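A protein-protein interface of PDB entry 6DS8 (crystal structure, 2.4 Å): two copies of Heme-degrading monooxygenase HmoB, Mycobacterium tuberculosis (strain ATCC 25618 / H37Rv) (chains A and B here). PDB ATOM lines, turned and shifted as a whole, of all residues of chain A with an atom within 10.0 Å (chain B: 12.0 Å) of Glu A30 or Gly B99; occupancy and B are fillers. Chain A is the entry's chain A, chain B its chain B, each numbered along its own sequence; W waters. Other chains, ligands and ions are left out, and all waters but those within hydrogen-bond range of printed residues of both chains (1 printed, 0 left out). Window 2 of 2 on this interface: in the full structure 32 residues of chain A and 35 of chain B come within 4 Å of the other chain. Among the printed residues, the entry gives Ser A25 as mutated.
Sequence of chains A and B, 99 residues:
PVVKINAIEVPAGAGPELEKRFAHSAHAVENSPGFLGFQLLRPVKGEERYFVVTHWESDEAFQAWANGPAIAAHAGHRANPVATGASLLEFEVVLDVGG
Among the printed residues, no Asp or Glu carboxylate lies within 4 Å of a Lys or Arg side-chain nitrogen of the other chain.
No position is printed for both chains.
Of the 12 pairs that touch across the chains among the printed residues, none has its exchanged pair printed and touching as well.
NE2 of Gln A39 is in hydrogen-bond range of OD2 of Asp B96.
The backbone NH (N) of Phe A38 is in hydrogen-bond range of the backbone carbonyl oxygen (O) of Val B97, 2.8 Å away.
No residue of chain B comes within 4 Å of Ala A28.
Val A29 touches none of the printed residues of chain B.
Of chain B, only Val B97, Gly B98 and Gly B99 come within 4 Å of Glu A30.
Gly A37 touches one residue of chain B.
Printed residues of chain B within 4 Å of Phe A38: Leu B95 (3.7 Å), Asp B96 (3.7 Å) and Val B97 (2.8 Å).
Of the printed residues of chain B, Gln A39 touches Leu B95 and Asp B96.
Printed residues of chain A within 4 Å of Leu B95: Phe A38 (3.7 Å) and Gln A39 (3.0 Å).
Printed residues of chain A within 4 Å of Asp B96: Phe A38 (3.7 Å) and Gln A39 (2.9 Å).
Printed residues of chain A within 4 Å of Val B97: Ala A26 (3.9 Å), Glu A30 (3.4 Å), Gly A37 (3.1 Å) and Phe A38 (2.8 Å).
Of the printed residues of chain A, Gly B98 touches Glu A30 (3.7 Å) and Phe A35 (3.7 Å).
Of chain A, only Glu A30 (3.0 Å) and Phe A35 (3.7 Å) come within 4 Å of Gly B99.
The nearest residue of chain B that does not touch Glu A30 is Asp B96 (7.0 Å).
The nearest printed residue of chain A that does not touch Gly B99 is Gly A37 (4.1 Å).
The nearest printed residue of chain B that does not touch Phe A38 is Gly B98 (5.0 Å).
Water W1 lies within hydrogen-bond range of ND2 of Asn A31 (2.8 Å), O of Gly B99 (3.0 Å) and O of Glu A30 (3.3 Å).
The backbone carbonyl oxygen (O) of Gly A37 sits at hydrogen-bond distance from the backbone NH (N) of His A55.
Ala A26 touches Val B97 (CB to CG1, 3.9 Å).
Val B97 touches Glu A30.
Gly B98 touches Glu A30.
Glu A30 touches Gly B99 (O to C, 3.0 Å).
Gly B98 touches Phe A35 (O to CE2, 3.7 Å).
Gly B99 touches Phe A35 (CA to O, 3.7 Å).
Gly A37 touches Val B97.
Leu B95 touches Phe A38 (CD2 to CZ, 3.7 Å).
Phe A38 touches Asp B96.
Leu B95 touches Gln A39.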
ATOM      1  N   ALA A  23     -28.886  -2.390 -29.324  1.00  0.00           N
ATOM      2  CA  ALA A  23     -28.773  -2.638 -30.758  1.00  0.00           C
ATOM      3  C   ALA A  23     -28.920  -1.386 -31.623  1.00  0.00           C
ATOM      4  O   ALA A  23     -28.293  -1.299 -32.685  1.00  0.00           O
ATOM      5  CB  ALA A  23     -29.817  -3.682 -31.162  1.00  0.00           C
ATOM      6  N   HIS A  24     -29.720  -0.411 -31.206  1.00  0.00           N
ATOM      7  CA  HIS A  24     -29.961   0.782 -32.005  1.00  0.00           C
ATOM      8  C   HIS A  24     -29.534   2.062 -31.285  1.00  0.00           C
ATOM      9  O   HIS A  24     -30.139   3.137 -31.437  1.00  0.00           O
ATOM     10  CB  HIS A  24     -31.420   0.804 -32.461  1.00  0.00           C
ATOM     11  CG  HIS A  24     -31.744  -0.331 -33.388  1.00  0.00           C
ATOM     12  ND1 HIS A  24     -32.711  -1.277 -33.116  1.00  0.00           N
ATOM     13  CD2 HIS A  24     -31.171  -0.709 -34.557  1.00  0.00           C
ATOM     14  CE1 HIS A  24     -32.741  -2.171 -34.094  1.00  0.00           C
ATOM     15  NE2 HIS A  24     -31.816  -1.849 -34.980  1.00  0.00           N
ATOM     16  N   SER A  25     -28.445   1.969 -30.530  1.00  0.00           N
ATOM     17  CA  SER A  25     -27.998   3.064 -29.696  1.00  0.00           C
ATOM     18  C   SER A  25     -26.859   3.862 -30.328  1.00  0.00           C
ATOM     19  O   SER A  25     -26.415   4.853 -29.733  1.00  0.00           O
ATOM     20  CB  SER A  25     -27.569   2.522 -28.327  1.00  0.00           C
ATOM     21  OG  SER A  25     -26.414   1.701 -28.413  1.00  0.00           O
ATOM     22  N   ALA A  26     -26.397   3.467 -31.529  1.00  0.00           N
ATOM     23  CA  ALA A  26     -25.243   4.114 -32.155  1.00  0.00           C
ATOM     24  C   ALA A  26     -25.385   5.635 -32.211  1.00  0.00           C
ATOM     25  O   ALA A  26     -24.422   6.363 -31.957  1.00  0.00           O
ATOM     26  CB  ALA A  26     -25.049   3.568 -33.572  1.00  0.00           C
ATOM     27  N   HIS A  27     -26.590   6.126 -32.529  1.00  0.00           N
ATOM     28  CA  HIS A  27     -26.823   7.550 -32.745  1.00  0.00           C
ATOM     29  C   HIS A  27     -26.462   8.396 -31.525  1.00  0.00           C
ATOM     30  O   HIS A  27     -26.136   9.577 -31.665  1.00  0.00           O
ATOM     31  CB  HIS A  27     -28.290   7.772 -33.138  1.00  0.00           C
ATOM     32  CG  HIS A  27     -29.259   7.465 -32.032  1.00  0.00           C
ATOM     33  ND1 HIS A  27     -29.931   8.448 -31.331  1.00  0.00           N
ATOM     34  CD2 HIS A  27     -29.643   6.285 -31.488  1.00  0.00           C
ATOM     35  CE1 HIS A  27     -30.697   7.886 -30.413  1.00  0.00           C
ATOM     36  NE2 HIS A  27     -30.542   6.573 -30.485  1.00  0.00           N
ATOM     37  N   ALA A  28     -26.545   7.816 -30.328  1.00  0.00           N
ATOM     38  CA  ALA A  28     -26.394   8.533 -29.069  1.00  0.00           C
ATOM     39  C   ALA A  28     -24.955   8.936 -28.769  1.00  0.00           C
ATOM     40  O   ALA A  28     -24.720   9.677 -27.811  1.00  0.00           O
ATOM     41  CB  ALA A  28     -26.946   7.674 -27.926  1.00  0.00           C
ATOM     42  N   VAL A  29     -23.984   8.397 -29.485  1.00  0.00           N
ATOM     43  CA  VAL A  29     -22.586   8.622 -29.143  1.00  0.00           C
ATOM     44  C   VAL A  29     -21.742   8.787 -30.410  1.00  0.00           C
ATOM     45  O   VAL A  29     -20.603   9.265 -30.359  1.00  0.00           O
ATOM     46  CB  VAL A  29     -22.077   7.471 -28.249  1.00  0.00           C
ATOM     47  CG1 VAL A  29     -21.946   6.170 -29.078  1.00  0.00           C
ATOM     48  CG2 VAL A  29     -20.787   7.862 -27.540  1.00  0.00           C
ATOM     49  N   GLU A  30     -22.294   8.376 -31.552  1.00  0.00           N
ATOM     50  CA  GLU A  30     -21.497   8.228 -32.768  1.00  0.00           C
ATOM     51  C   GLU A  30     -20.826   9.529 -33.180  1.00  0.00           C
ATOM     52  O   GLU A  30     -19.700   9.524 -33.697  1.00  0.00           O
ATOM     53  CB  GLU A  30     -22.400   7.786 -33.907  1.00  0.00           C
ATOM     54  CG  GLU A  30     -22.087   6.448 -34.440  1.00  0.00           C
ATOM     55  CD  GLU A  30     -23.002   6.107 -35.575  1.00  0.00           C
ATOM     56  OE1 GLU A  30     -24.112   6.702 -35.648  1.00  0.00           O
ATOM     57  OE2 GLU A  30     -22.589   5.270 -36.394  1.00  0.00           O
ATOM     58  N   ASN A  31     -21.511  10.649 -32.987  1.00  0.00           N
ATOM     59  CA  ASN A  31     -21.039  11.917 -33.508  1.00  0.00           C
ATOM     60  C   ASN A  31     -20.383  12.790 -32.431  1.00  0.00           C
ATOM     61  O   ASN A  31     -20.203  13.988 -32.651  1.00  0.00           O
ATOM     62  CB  ASN A  31     -22.213  12.625 -34.201  1.00  0.00           C
ATOM     63  CG  ASN A  31     -22.851  11.748 -35.314  1.00  0.00           C
ATOM     64  OD1 ASN A  31     -24.094  11.663 -35.436  1.00  0.00           O
ATOM     65  ND2 ASN A  31     -22.003  11.125 -36.143  1.00  0.00           N
ATOM     66  N   SER A  32     -20.024  12.211 -31.274  1.00  0.00           N
ATOM     67  CA  SER A  32     -19.377  12.981 -30.205  1.00  0.00           C
ATOM     68  C   SER A  32     -17.927  13.333 -30.540  1.00  0.00           C
ATOM     69  O   SER A  32     -17.172  12.489 -31.041  1.00  0.00           O
ATOM     70  CB  SER A  32     -19.418  12.216 -28.884  1.00  0.00           C
ATOM     71  OG  SER A  32     -20.742  12.178 -28.401  1.00  0.00           O
ATOM     72  N   PRO A  33     -17.506  14.560 -30.232  1.00  0.00           N
ATOM     73  CA  PRO A  33     -16.097  14.948 -30.400  1.00  0.00           C
ATOM     74  C   PRO A  33     -15.167  14.088 -29.555  1.00  0.00           C
ATOM     75  O   PRO A  33     -15.408  13.869 -28.366  1.00  0.00           O
ATOM     76  CB  PRO A  33     -16.081  16.408 -29.935  1.00  0.00           C
ATOM     77  CG  PRO A  33     -17.529  16.813 -29.823  1.00  0.00           C
ATOM     78  CD  PRO A  33     -18.276  15.579 -29.502  1.00  0.00           C
ATOM     79  N   GLY A  34     -14.077  13.627 -30.164  1.00  0.00           N
ATOM     80  CA  GLY A  34     -13.079  12.844 -29.465  1.00  0.00           C
ATOM     81  C   GLY A  34     -13.463  11.401 -29.234  1.00  0.00           C
ATOM     82  O   GLY A  34     -12.634  10.622 -28.737  1.00  0.00           O
ATOM     83  N   PHE A  35     -14.675  11.006 -29.609  1.00  0.00           N
ATOM     84  CA  PHE A  35     -15.095   9.626 -29.464  1.00  0.00           C
ATOM     85  C   PHE A  35     -14.432   8.797 -30.547  1.00  0.00           C
ATOM     86  O   PHE A  35     -14.513   9.133 -31.733  1.00  0.00           O
ATOM     87  CB  PHE A  35     -16.610   9.521 -29.570  1.00  0.00           C
ATOM     88  CG  PHE A  35     -17.121   8.115 -29.697  1.00  0.00           C
ATOM     89  CD1 PHE A  35     -17.173   7.277 -28.589  1.00  0.00           C
ATOM     90  CD2 PHE A  35     -17.599   7.641 -30.922  1.00  0.00           C
ATOM     91  CE1 PHE A  35     -17.664   5.984 -28.697  1.00  0.00           C
ATOM     92  CE2 PHE A  35     -18.112   6.349 -31.049  1.00  0.00           C
ATOM     93  CZ  PHE A  35     -18.148   5.519 -29.930  1.00  0.00           C
ATOM     94  N   LEU A  36     -13.789   7.706 -30.146  1.00  0.00           N
ATOM     95  CA  LEU A  36     -13.067   6.878 -31.098  1.00  0.00           C
ATOM     96  C   LEU A  36     -13.740   5.541 -31.364  1.00  0.00           C
ATOM     97  O   LEU A  36     -13.187   4.750 -32.120  1.00  0.00           O
ATOM     98  CB  LEU A  36     -11.625   6.641 -30.627  1.00  0.00           C
ATOM     99  CG  LEU A  36     -10.770   7.914 -30.544  1.00  0.00           C
ATOM    100  CD1 LEU A  36      -9.409   7.572 -29.994  1.00  0.00           C
ATOM    101  CD2 LEU A  36     -10.680   8.624 -31.906  1.00  0.00           C
ATOM    102  N   GLY A  37     -14.912   5.277 -30.806  1.00  0.00           N
ATOM    103  CA  GLY A  37     -15.606   4.024 -31.054  1.00  0.00           C
ATOM    104  C   GLY A  37     -15.958   3.289 -29.781  1.00  0.00           C
ATOM    105  O   GLY A  37     -15.474   3.591 -28.687  1.00  0.00           O
ATOM    106  N   PHE A  38     -16.826   2.286 -29.937  1.00  0.00           N
ATOM    107  CA  PHE A  38     -17.173   1.457 -28.798  1.00  0.00           C
ATOM    108  C   PHE A  38     -17.691   0.114 -29.268  1.00  0.00           C
ATOM    109  O   PHE A  38     -18.212  -0.009 -30.375  1.00  0.00           O
ATOM    110  CB  PHE A  38     -18.196   2.162 -27.881  1.00  0.00           C
ATOM    111  CG  PHE A  38     -19.633   1.784 -28.104  1.00  0.00           C
ATOM    112  CD1 PHE A  38     -20.419   2.496 -28.995  1.00  0.00           C
ATOM    113  CD2 PHE A  38     -20.241   0.794 -27.332  1.00  0.00           C
ATOM    114  CE1 PHE A  38     -21.759   2.191 -29.158  1.00  0.00           C
ATOM    115  CE2 PHE A  38     -21.592   0.485 -27.491  1.00  0.00           C
ATOM    116  CZ  PHE A  38     -22.341   1.185 -28.404  1.00  0.00           C
ATOM    117  N   GLN A  39     -17.534  -0.891 -28.413  1.00  0.00           N
ATOM    118  CA  GLN A  39     -18.046  -2.224 -28.698  1.00  0.00           C
ATOM    119  C   GLN A  39     -18.904  -2.684 -27.531  1.00  0.00           C
ATOM    120  O   GLN A  39     -18.565  -2.425 -26.373  1.00  0.00           O
ATOM    121  CB  GLN A  39     -16.928  -3.278 -28.932  1.00  0.00           C
ATOM    122  CG  GLN A  39     -15.742  -2.846 -29.790  1.00  0.00           C
ATOM    123  CD  GLN A  39     -14.663  -3.971 -29.922  1.00  0.00           C
ATOM    124  OE1 GLN A  39     -13.899  -4.271 -28.973  1.00  0.00           O
ATOM    125  NE2 GLN A  39     -14.611  -4.592 -31.102  1.00  0.00           N
ATOM    126  N   THR A  54     -15.477   1.617 -24.516  1.00  0.00           N
ATOM    127  CA  THR A  54     -15.453   2.881 -25.246  1.00  0.00           C
ATOM    128  C   THR A  54     -14.041   3.458 -25.251  1.00  0.00           C
ATOM    129  O   THR A  54     -13.303   3.345 -24.257  1.00  0.00           O
ATOM    130  CB  THR A  54     -16.448   3.902 -24.661  1.00  0.00           C
ATOM    131  OG1 THR A  54     -15.951   4.469 -23.432  1.00  0.00           O
ATOM    132  CG2 THR A  54     -17.808   3.222 -24.424  1.00  0.00           C
ATOM    133  N   HIS A  55     -13.667   4.042 -26.401  1.00  0.00           N
ATOM    134  CA  HIS A  55     -12.351   4.623 -26.645  1.00  0.00           C
ATOM    135  C   HIS A  55     -12.527   6.112 -26.884  1.00  0.00           C
ATOM    136  O   HIS A  55     -13.447   6.527 -27.602  1.00  0.00           O
ATOM    137  CB  HIS A  55     -11.645   4.012 -27.867  1.00  0.00           C
ATOM    138  CG  HIS A  55     -11.543   2.520 -27.829  1.00  0.00           C
ATOM    139  ND1 HIS A  55     -12.648   1.693 -27.923  1.00  0.00           N
ATOM    140  CD2 HIS A  55     -10.467   1.703 -27.717  1.00  0.00           C
ATOM    141  CE1 HIS A  55     -12.256   0.430 -27.868  1.00  0.00           C
ATOM    142  NE2 HIS A  55     -10.936   0.408 -27.747  1.00  0.00           N
ATOM    143  N   TRP A  56     -11.666   6.923 -26.278  1.00  0.00           N
ATOM    144  CA  TRP A  56     -11.787   8.370 -26.437  1.00  0.00           C
ATOM    145  C   TRP A  56     -10.405   8.973 -26.608  1.00  0.00           C
ATOM    146  O   TRP A  56      -9.398   8.448 -26.100  1.00  0.00           O
ATOM    147  CB  TRP A  56     -12.501   9.058 -25.258  1.00  0.00           C
ATOM    148  CG  TRP A  56     -13.795   8.447 -24.953  1.00  0.00           C
ATOM    149  CD1 TRP A  56     -14.004   7.230 -24.332  1.00  0.00           C
ATOM    150  CD2 TRP A  56     -15.096   8.979 -25.238  1.00  0.00           C
ATOM    151  NE1 TRP A  56     -15.344   6.981 -24.232  1.00  0.00           N
ATOM    152  CE2 TRP A  56     -16.047   8.029 -24.766  1.00  0.00           C
ATOM    153  CE3 TRP A  56     -15.556  10.163 -25.833  1.00  0.00           C
ATOM    154  CZ2 TRP A  56     -17.432   8.228 -24.869  1.00  0.00           C
ATOM    155  CZ3 TRP A  56     -16.945  10.362 -25.938  1.00  0.00           C
ATOM    156  CH2 TRP A  56     -17.860   9.390 -25.465  1.00  0.00           C
ATOM    157  N   GLU A  57     -10.375  10.082 -27.354  1.00  0.00           N
ATOM    158  CA  GLU A  57      -9.136  10.829 -27.523  1.00  0.00           C
ATOM    159  C   GLU A  57      -8.612  11.305 -26.176  1.00  0.00           C
ATOM    160  O   GLU A  57      -7.392  11.327 -25.951  1.00  0.00           O
ATOM    161  CB  GLU A  57      -9.345  11.986 -28.505  1.00  0.00           C
ATOM    162  CG  GLU A  57      -8.051  12.657 -28.936  1.00  0.00           C
ATOM    163  CD  GLU A  57      -6.982  11.674 -29.488  1.00  0.00           C
ATOM    164  OE1 GLU A  57      -7.259  10.955 -30.490  1.00  0.00           O
ATOM    165  OE2 GLU A  57      -5.863  11.627 -28.904  1.00  0.00           O
ATOM    166  N   TRP A  65     -19.331  14.002 -23.074  1.00  0.00           N
ATOM    167  CA  TRP A  65     -20.450  13.198 -23.555  1.00  0.00           C
ATOM    168  C   TRP A  65     -21.294  12.687 -22.400  1.00  0.00           C
ATOM    169  O   TRP A  65     -22.530  12.765 -22.443  1.00  0.00           O
ATOM    170  CB  TRP A  65     -19.932  12.031 -24.399  1.00  0.00           C
ATOM    171  CG  TRP A  65     -20.998  11.094 -24.807  1.00  0.00           C
ATOM    172  CD1 TRP A  65     -21.947  11.307 -25.754  1.00  0.00           C
ATOM    173  CD2 TRP A  65     -21.254   9.788 -24.257  1.00  0.00           C
ATOM    174  NE1 TRP A  65     -22.783  10.214 -25.844  1.00  0.00           N
ATOM    175  CE2 TRP A  65     -22.378   9.265 -24.938  1.00  0.00           C
ATOM    176  CE3 TRP A  65     -20.641   9.013 -23.263  1.00  0.00           C
ATOM    177  CZ2 TRP A  65     -22.910   8.002 -24.653  1.00  0.00           C
ATOM    178  CZ3 TRP A  65     -21.160   7.740 -22.988  1.00  0.00           C
ATOM    179  CH2 TRP A  65     -22.289   7.255 -23.677  1.00  0.00           C
ATOM    180  N   PRO A  69     -25.011  14.999 -23.763  1.00  0.00           N
ATOM    181  CA  PRO A  69     -25.723  14.154 -24.746  1.00  0.00           C
ATOM    182  C   PRO A  69     -26.202  12.829 -24.180  1.00  0.00           C
ATOM    183  O   PRO A  69     -27.325  12.396 -24.478  1.00  0.00           O
ATOM    184  CB  PRO A  69     -24.671  13.963 -25.852  1.00  0.00           C
ATOM    185  CG  PRO A  69     -23.841  15.216 -25.766  1.00  0.00           C
ATOM    186  CD  PRO A  69     -23.782  15.598 -24.313  1.00  0.00           C
ATOM    187  N   ALA A  70     -25.355  12.163 -23.385  1.00  0.00           N
ATOM    188  CA  ALA A  70     -25.703  10.856 -22.845  1.00  0.00           C
ATOM    189  C   ALA A  70     -26.975  10.929 -22.004  1.00  0.00           C
ATOM    190  O   ALA A  70     -27.872  10.083 -22.152  1.00  0.00           O
ATOM    191  CB  ALA A  70     -24.527  10.303 -22.033  1.00  0.00           C
ATOM    192  N   ALA A  73     -29.942  11.647 -24.330  1.00  0.00           N
ATOM    193  CA  ALA A  73     -30.365  10.520 -25.170  1.00  0.00           C
ATOM    194  C   ALA A  73     -31.374   9.599 -24.484  1.00  0.00           C
ATOM    195  O   ALA A  73     -31.847   8.633 -25.091  1.00  0.00           O
ATOM    196  CB  ALA A  73     -29.155   9.699 -25.632  1.00  0.00           C
ATOM    197  N   LEU B  95     -21.669  -5.798 -30.864  1.00  0.00           N
ATOM    198  CA  LEU B  95     -21.946  -4.524 -31.506  1.00  0.00           C
ATOM    199  C   LEU B  95     -20.660  -3.710 -31.610  1.00  0.00           C
ATOM    200  O   LEU B  95     -19.917  -3.599 -30.634  1.00  0.00           O
ATOM    201  CB  LEU B  95     -23.017  -3.778 -30.713  1.00  0.00           C
ATOM    202  CG  LEU B  95     -23.334  -2.416 -31.262  1.00  0.00           C
ATOM    203  CD1 LEU B  95     -24.226  -2.660 -32.462  1.00  0.00           C
ATOM    204  CD2 LEU B  95     -24.024  -1.602 -30.149  1.00  0.00           C
ATOM    205  N   ASP B  96     -20.388  -3.159 -32.789  1.00  0.00           N
ATOM    206  CA  ASP B  96     -19.185  -2.373 -33.028  1.00  0.00           C
ATOM    207  C   ASP B  96     -19.579  -1.075 -33.723  1.00  0.00           C
ATOM    208  O   ASP B  96     -20.215  -1.109 -34.785  1.00  0.00           O
ATOM    209  CB  ASP B  96     -18.167  -3.180 -33.852  1.00  0.00           C
ATOM    210  CG  ASP B  96     -16.737  -2.690 -33.646  1.00  0.00           C
ATOM    211  OD1 ASP B  96     -16.583  -1.465 -33.530  1.00  0.00           O
ATOM    212  OD2 ASP B  96     -15.781  -3.500 -33.564  1.00  0.00           O
ATOM    213  N   VAL B  97     -19.265   0.062 -33.089  1.00  0.00           N
ATOM    214  CA  VAL B  97     -19.677   1.388 -33.548  1.00  0.00           C
ATOM    215  C   VAL B  97     -18.425   2.254 -33.601  1.00  0.00           C
ATOM    216  O   VAL B  97     -17.700   2.354 -32.604  1.00  0.00           O
ATOM    217  CB  VAL B  97     -20.733   2.012 -32.606  1.00  0.00           C
ATOM    218  CG1 VAL B  97     -21.160   3.446 -33.041  1.00  0.00           C
ATOM    219  CG2 VAL B  97     -21.937   1.130 -32.489  1.00  0.00           C
ATOM    220  N   GLY B  98     -18.158   2.870 -34.764  1.00  0.00           N
ATOM    221  CA  GLY B  98     -16.992   3.713 -34.931  1.00  0.00           C
ATOM    222  C   GLY B  98     -17.293   5.186 -34.725  1.00  0.00           C
ATOM    223  O   GLY B  98     -18.443   5.612 -34.677  1.00  0.00           O
ATOM    224  N   GLY B  99     -16.218   5.971 -34.649  1.00  0.00           N
ATOM    225  CA  GLY B  99     -16.288   7.418 -34.446  1.00  0.00           C
ATOM    226  C   GLY B  99     -17.399   8.183 -35.154  1.00  0.00           C
ATOM    227  O   GLY B  99     -17.400   8.338 -36.379  1.00  0.00           O
HETATM  228  O   HOH W   1     -19.243  10.697 -36.704  1.00  0.00           O
